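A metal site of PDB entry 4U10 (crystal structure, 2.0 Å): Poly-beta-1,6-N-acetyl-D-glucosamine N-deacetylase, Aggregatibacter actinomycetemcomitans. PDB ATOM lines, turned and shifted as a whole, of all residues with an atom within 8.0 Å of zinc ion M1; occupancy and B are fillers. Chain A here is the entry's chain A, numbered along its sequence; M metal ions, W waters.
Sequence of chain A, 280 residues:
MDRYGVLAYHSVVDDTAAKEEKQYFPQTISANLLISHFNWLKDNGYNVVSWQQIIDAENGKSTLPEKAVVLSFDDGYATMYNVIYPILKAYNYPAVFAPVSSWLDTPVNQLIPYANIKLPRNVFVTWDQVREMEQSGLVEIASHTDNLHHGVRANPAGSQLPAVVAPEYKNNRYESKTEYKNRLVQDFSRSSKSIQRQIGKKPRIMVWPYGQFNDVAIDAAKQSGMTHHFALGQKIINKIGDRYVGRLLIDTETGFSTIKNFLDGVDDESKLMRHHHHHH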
ATOM      1  N   TYR A   9       5.881   6.326 -15.529  1.00  0.00           N
ATOM      2  CA  TYR A   9       5.939   5.607 -16.787  1.00  0.00           C
ATOM      3  C   TYR A   9       6.801   4.354 -16.609  1.00  0.00           C
ATOM      4  O   TYR A   9       7.524   4.275 -15.657  1.00  0.00           O
ATOM      5  CB  TYR A   9       6.628   6.432 -17.881  1.00  0.00           C
ATOM      6  CG  TYR A   9       5.802   7.617 -18.399  1.00  0.00           C
ATOM      7  CD1 TYR A   9       4.912   7.482 -19.460  1.00  0.00           C
ATOM      8  CD2 TYR A   9       5.974   8.886 -17.843  1.00  0.00           C
ATOM      9  CE1 TYR A   9       4.147   8.580 -19.883  1.00  0.00           C
ATOM     10  CE2 TYR A   9       5.246  10.001 -18.301  1.00  0.00           C
ATOM     11  CZ  TYR A   9       4.358   9.857 -19.274  1.00  0.00           C
ATOM     12  OH  TYR A   9       3.622  10.995 -19.677  1.00  0.00           O
ATOM     13  N   HIS A  10       6.682   3.391 -17.525  1.00  0.00           N
ATOM     14  CA  HIS A  10       7.554   2.205 -17.536  1.00  0.00           C
ATOM     15  C   HIS A  10       8.220   2.155 -18.897  1.00  0.00           C
ATOM     16  O   HIS A  10       9.022   3.076 -19.233  1.00  0.00           O
ATOM     17  CB  HIS A  10       6.712   0.967 -17.168  1.00  0.00           C
ATOM     18  CG  HIS A  10       6.258   1.009 -15.748  1.00  0.00           C
ATOM     19  ND1 HIS A  10       5.187   1.782 -15.352  1.00  0.00           N
ATOM     20  CD2 HIS A  10       6.790   0.501 -14.635  1.00  0.00           C
ATOM     21  CE1 HIS A  10       5.043   1.710 -14.048  1.00  0.00           C
ATOM     22  NE2 HIS A  10       6.000   0.927 -13.579  1.00  0.00           N
ATOM     23  N   PHE A  73      10.413   7.162 -14.631  1.00  0.00           N
ATOM     24  CA  PHE A  73      10.437   5.984 -15.479  1.00  0.00           C
ATOM     25  C   PHE A  73      11.013   4.851 -14.673  1.00  0.00           C
ATOM     26  O   PHE A  73      12.065   5.005 -14.021  1.00  0.00           O
ATOM     27  CB  PHE A  73      11.239   6.192 -16.750  1.00  0.00           C
ATOM     28  CG  PHE A  73      10.705   7.290 -17.619  1.00  0.00           C
ATOM     29  CD1 PHE A  73      11.071   8.625 -17.381  1.00  0.00           C
ATOM     30  CD2 PHE A  73       9.876   7.008 -18.690  1.00  0.00           C
ATOM     31  CE1 PHE A  73      10.522   9.641 -18.175  1.00  0.00           C
ATOM     32  CE2 PHE A  73       9.359   8.012 -19.468  1.00  0.00           C
ATOM     33  CZ  PHE A  73       9.665   9.326 -19.198  1.00  0.00           C
ATOM     34  N   ASP A  74      10.234   3.780 -14.569  1.00  0.00           N
ATOM     35  CA  ASP A  74      10.583   2.632 -13.732  1.00  0.00           C
ATOM     36  C   ASP A  74      11.082   1.414 -14.524  1.00  0.00           C
ATOM     37  O   ASP A  74      10.533   1.081 -15.568  1.00  0.00           O
ATOM     38  CB  ASP A  74       9.395   2.102 -12.941  1.00  0.00           C
ATOM     39  CG  ASP A  74       8.837   3.058 -11.889  1.00  0.00           C
ATOM     40  OD1 ASP A  74       9.386   4.153 -11.643  1.00  0.00           O
ATOM     41  OD2 ASP A  74       7.819   2.620 -11.252  1.00  0.00           O
ATOM     42  N   ASP A  75      12.128   0.776 -13.942  1.00  0.00           N
ATOM     43  CA  ASP A  75      12.501  -0.631 -14.037  1.00  0.00           C
ATOM     44  C   ASP A  75      13.879  -0.888 -14.634  1.00  0.00           C
ATOM     45  O   ASP A  75      14.482  -1.867 -14.286  1.00  0.00           O
ATOM     46  CB  ASP A  75      11.501  -1.512 -14.790  1.00  0.00           C
ATOM     47  CG  ASP A  75      10.280  -1.762 -14.019  1.00  0.00           C
ATOM     48  OD1 ASP A  75      10.037  -1.147 -12.979  1.00  0.00           O
ATOM     49  OD2 ASP A  75       9.533  -2.642 -14.478  1.00  0.00           O
ATOM     50  N   GLY A  76      14.382   0.024 -15.449  1.00  0.00           N
ATOM     51  CA  GLY A  76      15.671  -0.187 -16.129  1.00  0.00           C
ATOM     52  C   GLY A  76      15.570  -0.689 -17.526  1.00  0.00           C
ATOM     53  O   GLY A  76      16.578  -1.147 -18.055  1.00  0.00           O
ATOM     54  N   TYR A  77      14.393  -0.612 -18.158  1.00  0.00           N
ATOM     55  CA  TYR A  77      14.306  -1.083 -19.609  1.00  0.00           C
ATOM     56  C   TYR A  77      15.222  -0.315 -20.527  1.00  0.00           C
ATOM     57  O   TYR A  77      15.307   0.887 -20.403  1.00  0.00           O
ATOM     58  CB  TYR A  77      12.888  -1.030 -20.161  1.00  0.00           C
ATOM     59  CG  TYR A  77      11.859  -1.827 -19.392  1.00  0.00           C
ATOM     60  CD1 TYR A  77      11.931  -3.226 -19.280  1.00  0.00           C
ATOM     61  CD2 TYR A  77      10.820  -1.181 -18.740  1.00  0.00           C
ATOM     62  CE1 TYR A  77      10.956  -3.925 -18.554  1.00  0.00           C
ATOM     63  CE2 TYR A  77       9.898  -1.864 -18.067  1.00  0.00           C
ATOM     64  CZ  TYR A  77       9.949  -3.232 -17.960  1.00  0.00           C
ATOM     65  OH  TYR A  77       8.919  -3.855 -17.232  1.00  0.00           O
ATOM     66  N   ALA A  98      14.390   4.825 -12.387  1.00  0.00           N
ATOM     67  CA  ALA A  98      14.560   3.875 -11.312  1.00  0.00           C
ATOM     68  C   ALA A  98      14.806   2.436 -11.800  1.00  0.00           C
ATOM     69  O   ALA A  98      13.899   1.561 -11.856  1.00  0.00           O
ATOM     70  CB  ALA A  98      13.398   3.958 -10.362  1.00  0.00           C
ATOM     71  N   PRO A  99      16.077   2.174 -12.157  1.00  0.00           N
ATOM     72  CA  PRO A  99      16.396   0.814 -12.566  1.00  0.00           C
ATOM     73  C   PRO A  99      16.557  -0.170 -11.394  1.00  0.00           C
ATOM     74  O   PRO A  99      17.086   0.167 -10.340  1.00  0.00           O
ATOM     75  CB  PRO A  99      17.713   1.029 -13.345  1.00  0.00           C
ATOM     76  CG  PRO A  99      18.406   2.097 -12.469  1.00  0.00           C
ATOM     77  CD  PRO A  99      17.260   3.041 -12.138  1.00  0.00           C
ATOM     78  N   VAL A 100      16.105  -1.417 -11.557  1.00  0.00           N
ATOM     79  CA  VAL A 100      16.410  -2.411 -10.600  1.00  0.00           C
ATOM     80  C   VAL A 100      17.903  -2.719 -10.663  1.00  0.00           C
ATOM     81  O   VAL A 100      18.391  -3.188 -11.672  1.00  0.00           O
ATOM     82  CB  VAL A 100      15.601  -3.659 -10.861  1.00  0.00           C
ATOM     83  CG1 VAL A 100      15.961  -4.729  -9.814  1.00  0.00           C
ATOM     84  CG2 VAL A 100      14.080  -3.368 -10.824  1.00  0.00           C
ATOM     85  N   TRP A 103      19.467  -6.234 -11.783  1.00  0.00           N
ATOM     86  CA  TRP A 103      19.268  -6.474 -13.210  1.00  0.00           C
ATOM     87  C   TRP A 103      20.443  -5.827 -13.973  1.00  0.00           C
ATOM     88  O   TRP A 103      21.129  -6.494 -14.755  1.00  0.00           O
ATOM     89  CB  TRP A 103      17.879  -5.962 -13.682  1.00  0.00           C
ATOM     90  CG  TRP A 103      16.765  -6.666 -13.097  1.00  0.00           C
ATOM     91  CD1 TRP A 103      16.832  -7.838 -12.320  1.00  0.00           C
ATOM     92  CD2 TRP A 103      15.388  -6.333 -13.205  1.00  0.00           C
ATOM     93  NE1 TRP A 103      15.568  -8.198 -11.957  1.00  0.00           N
ATOM     94  CE2 TRP A 103      14.668  -7.293 -12.475  1.00  0.00           C
ATOM     95  CE3 TRP A 103      14.673  -5.278 -13.822  1.00  0.00           C
ATOM     96  CZ2 TRP A 103      13.289  -7.266 -12.383  1.00  0.00           C
ATOM     97  CZ3 TRP A 103      13.296  -5.244 -13.718  1.00  0.00           C
ATOM     98  CH2 TRP A 103      12.625  -6.235 -13.030  1.00  0.00           C
ATOM     99  N   TYR A 114      13.264 -14.089 -13.868  1.00  0.00           N
ATOM    100  CA  TYR A 114      12.143 -13.171 -13.726  1.00  0.00           C
ATOM    101  C   TYR A 114      10.836 -13.976 -13.705  1.00  0.00           C
ATOM    102  O   TYR A 114      10.354 -14.402 -14.759  1.00  0.00           O
ATOM    103  CB  TYR A 114      12.164 -12.176 -14.876  1.00  0.00           C
ATOM    104  CG  TYR A 114      11.257 -10.975 -14.742  1.00  0.00           C
ATOM    105  CD1 TYR A 114       9.858 -11.087 -14.782  1.00  0.00           C
ATOM    106  CD2 TYR A 114      11.800  -9.703 -14.670  1.00  0.00           C
ATOM    107  CE1 TYR A 114       9.030  -9.978 -14.686  1.00  0.00           C
ATOM    108  CE2 TYR A 114      10.981  -8.583 -14.599  1.00  0.00           C
ATOM    109  CZ  TYR A 114       9.613  -8.714 -14.601  1.00  0.00           C
ATOM    110  OH  TYR A 114       8.868  -7.575 -14.524  1.00  0.00           O
ATOM    111  N   HIS A 144      15.106   1.232  -7.182  1.00  0.00           N
ATOM    112  CA  HIS A 144      13.879   0.465  -7.357  1.00  0.00           C
ATOM    113  C   HIS A 144      14.153  -0.931  -6.793  1.00  0.00           C
ATOM    114  O   HIS A 144      13.592  -1.936  -7.269  1.00  0.00           O
ATOM    115  CB  HIS A 144      13.561   0.375  -8.835  1.00  0.00           C
ATOM    116  CG  HIS A 144      12.138   0.082  -9.198  1.00  0.00           C
ATOM    117  ND1 HIS A 144      11.037   0.608  -8.539  1.00  0.00           N
ATOM    118  CD2 HIS A 144      11.638  -0.525 -10.294  1.00  0.00           C
ATOM    119  CE1 HIS A 144       9.948   0.269  -9.168  1.00  0.00           C
ATOM    120  NE2 HIS A 144      10.278  -0.402 -10.253  1.00  0.00           N
ATOM    121  N   THR A 145      14.909  -0.953  -5.681  1.00  0.00           N
ATOM    122  CA  THR A 145      15.408  -2.123  -4.929  1.00  0.00           C
ATOM    123  C   THR A 145      16.546  -2.740  -5.709  1.00  0.00           C
ATOM    124  O   THR A 145      16.768  -2.356  -6.826  1.00  0.00           O
ATOM    125  CB  THR A 145      14.343  -3.203  -4.563  1.00  0.00           C
ATOM    126  OG1 THR A 145      14.029  -3.936  -5.733  1.00  0.00           O
ATOM    127  CG2 THR A 145      13.055  -2.510  -4.067  1.00  0.00           C
ATOM    128  N   HIS A 149      12.131  -6.788  -6.805  1.00  0.00           N
ATOM    129  CA  HIS A 149      11.135  -6.479  -7.806  1.00  0.00           C
ATOM    130  C   HIS A 149      10.596  -7.799  -8.289  1.00  0.00           C
ATOM    131  O   HIS A 149      10.683  -8.117  -9.483  1.00  0.00           O
ATOM    132  CB  HIS A 149      11.781  -5.769  -8.958  1.00  0.00           C
ATOM    133  CG  HIS A 149      10.826  -4.991  -9.780  1.00  0.00           C
ATOM    134  ND1 HIS A 149       9.877  -5.554 -10.592  1.00  0.00           N
ATOM    135  CD2 HIS A 149      10.657  -3.648  -9.898  1.00  0.00           C
ATOM    136  CE1 HIS A 149       9.160  -4.622 -11.163  1.00  0.00           C
ATOM    137  NE2 HIS A 149       9.652  -3.449 -10.801  1.00  0.00           N
ATOM    138  N   VAL A 207      11.896   4.155  -5.272  1.00  0.00           N
ATOM    139  CA  VAL A 207      10.646   3.950  -5.960  1.00  0.00           C
ATOM    140  C   VAL A 207      10.151   2.551  -5.738  1.00  0.00           C
ATOM    141  O   VAL A 207      10.841   1.568  -6.075  1.00  0.00           O
ATOM    142  CB  VAL A 207      10.780   4.243  -7.470  1.00  0.00           C
ATOM    143  CG1 VAL A 207       9.414   4.121  -8.140  1.00  0.00           C
ATOM    144  CG2 VAL A 207      11.394   5.634  -7.738  1.00  0.00           C
ATOM    145  N   TRP A 208       8.911   2.410  -5.257  1.00  0.00           N
ATOM    146  CA  TRP A 208       8.434   1.068  -4.823  1.00  0.00           C
ATOM    147  C   TRP A 208       8.011   0.286  -6.026  1.00  0.00           C
ATOM    148  O   TRP A 208       7.247   0.826  -6.877  1.00  0.00           O
ATOM    149  CB  TRP A 208       7.228   1.228  -3.901  1.00  0.00           C
ATOM    150  CG  TRP A 208       7.521   2.059  -2.682  1.00  0.00           C
ATOM    151  CD1 TRP A 208       6.880   3.212  -2.319  1.00  0.00           C
ATOM    152  CD2 TRP A 208       8.483   1.788  -1.654  1.00  0.00           C
ATOM    153  NE1 TRP A 208       7.419   3.670  -1.146  1.00  0.00           N
ATOM    154  CE2 TRP A 208       8.407   2.825  -0.731  1.00  0.00           C
ATOM    155  CE3 TRP A 208       9.440   0.777  -1.452  1.00  0.00           C
ATOM    156  CZ2 TRP A 208       9.233   2.891   0.373  1.00  0.00           C
ATOM    157  CZ3 TRP A 208      10.232   0.848  -0.376  1.00  0.00           C
ATOM    158  CH2 TRP A 208      10.127   1.894   0.539  1.00  0.00           C
ATOM    159  N   PRO A 209       8.491  -0.972  -6.163  1.00  0.00           N
ATOM    160  CA  PRO A 209       7.910  -1.870  -7.167  1.00  0.00           C
ATOM    161  C   PRO A 209       6.407  -1.964  -7.030  1.00  0.00           C
ATOM    162  O   PRO A 209       5.896  -2.182  -5.905  1.00  0.00           O
ATOM    163  CB  PRO A 209       8.551  -3.240  -6.785  1.00  0.00           C
ATOM    164  CG  PRO A 209       9.933  -2.829  -6.383  1.00  0.00           C
ATOM    165  CD  PRO A 209       9.582  -1.669  -5.448  1.00  0.00           C
ATOM    166  N   TYR A 210       5.698  -1.804  -8.147  1.00  0.00           N
ATOM    167  CA  TYR A 210       4.249  -1.952  -8.231  1.00  0.00           C
ATOM    168  C   TYR A 210       3.542  -0.946  -7.358  1.00  0.00           C
ATOM    169  O   TYR A 210       2.385  -1.107  -7.056  1.00  0.00           O
ATOM    170  CB  TYR A 210       3.851  -3.394  -7.781  1.00  0.00           C
ATOM    171  CG  TYR A 210       4.789  -4.543  -8.266  1.00  0.00           C
ATOM    172  CD1 TYR A 210       4.911  -4.868  -9.579  1.00  0.00           C
ATOM    173  CD2 TYR A 210       5.520  -5.305  -7.348  1.00  0.00           C
ATOM    174  CE1 TYR A 210       5.763  -5.895  -9.991  1.00  0.00           C
ATOM    175  CE2 TYR A 210       6.338  -6.352  -7.750  1.00  0.00           C
ATOM    176  CZ  TYR A 210       6.458  -6.650  -9.078  1.00  0.00           C
ATOM    177  OH  TYR A 210       7.279  -7.699  -9.471  1.00  0.00           O
ATOM    178  N   GLY A 211       4.212   0.100  -6.886  1.00  0.00           N
ATOM    179  CA  GLY A 211       3.494   1.088  -6.058  1.00  0.00           C
ATOM    180  C   GLY A 211       3.327   0.657  -4.594  1.00  0.00           C
ATOM    181  O   GLY A 211       2.751   1.388  -3.823  1.00  0.00           O
ATOM    182  N   ARG A 247       2.097   9.349  -7.369  1.00  0.00           N
ATOM    183  CA  ARG A 247       2.292   9.412  -8.777  1.00  0.00           C
ATOM    184  C   ARG A 247       1.054   8.923  -9.505  1.00  0.00           C
ATOM    185  O   ARG A 247       0.295   8.053  -9.016  1.00  0.00           O
ATOM    186  CB  ARG A 247       3.526   8.570  -9.177  1.00  0.00           C
ATOM    187  CG  ARG A 247       4.852   8.903  -8.453  1.00  0.00           C
ATOM    188  CD  ARG A 247       6.006   8.176  -9.157  1.00  0.00           C
ATOM    189  NE  ARG A 247       5.867   6.701  -9.016  1.00  0.00           N
ATOM    190  CZ  ARG A 247       6.569   5.791  -9.679  1.00  0.00           C
ATOM    191  NH1 ARG A 247       7.476   6.155 -10.580  1.00  0.00           N
ATOM    192  NH2 ARG A 247       6.355   4.491  -9.488  1.00  0.00           N
HETATM  193 ZN    ZN M   1       9.018  -1.592 -11.437  1.00  0.00          ZN
HETATM  194 ZN    ZN M   2       6.653   0.912 -11.524  1.00  0.00          ZN
HETATM  195  O   HOH W   1       7.341  -2.910 -13.180  1.00  0.00           O
HETATM  196  O   HOH W   2       7.367  -0.863 -10.936  1.00  0.00           O
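Water W2 binds zinc ion M1. OD1 of Asp 75 is bound to zinc ion M1. NE2 of His 149 binds zinc ion M1 (2.1 Å). NE2 of His 144 is bound to zinc ion M1, 2.1 Å away. Slightly farther from zinc ion M1 lies water W1 (2.8 Å).
OH of Tyr 77 sits at hydrogen-bond distance from OD2 of Asp 75 (3.1 Å). The backbone carbonyl oxygen (O) of His 149 is in hydrogen-bond range of the side-chain hydroxyl (OH) of Tyr 210, at 3.4 Å. N of Asp 75 sits at hydrogen-bond distance from O of Ala 98 (2.8 Å). The backbone carbonyl oxygen (O) of Asp 75 lies within hydrogen-bond range of the backbone NH (N) of Val 100 (3.2 Å). A ring nitrogen (ND1) of His 144 is in hydrogen-bond range of the backbone carbonyl oxygen of Val 207 (2.7 Å).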
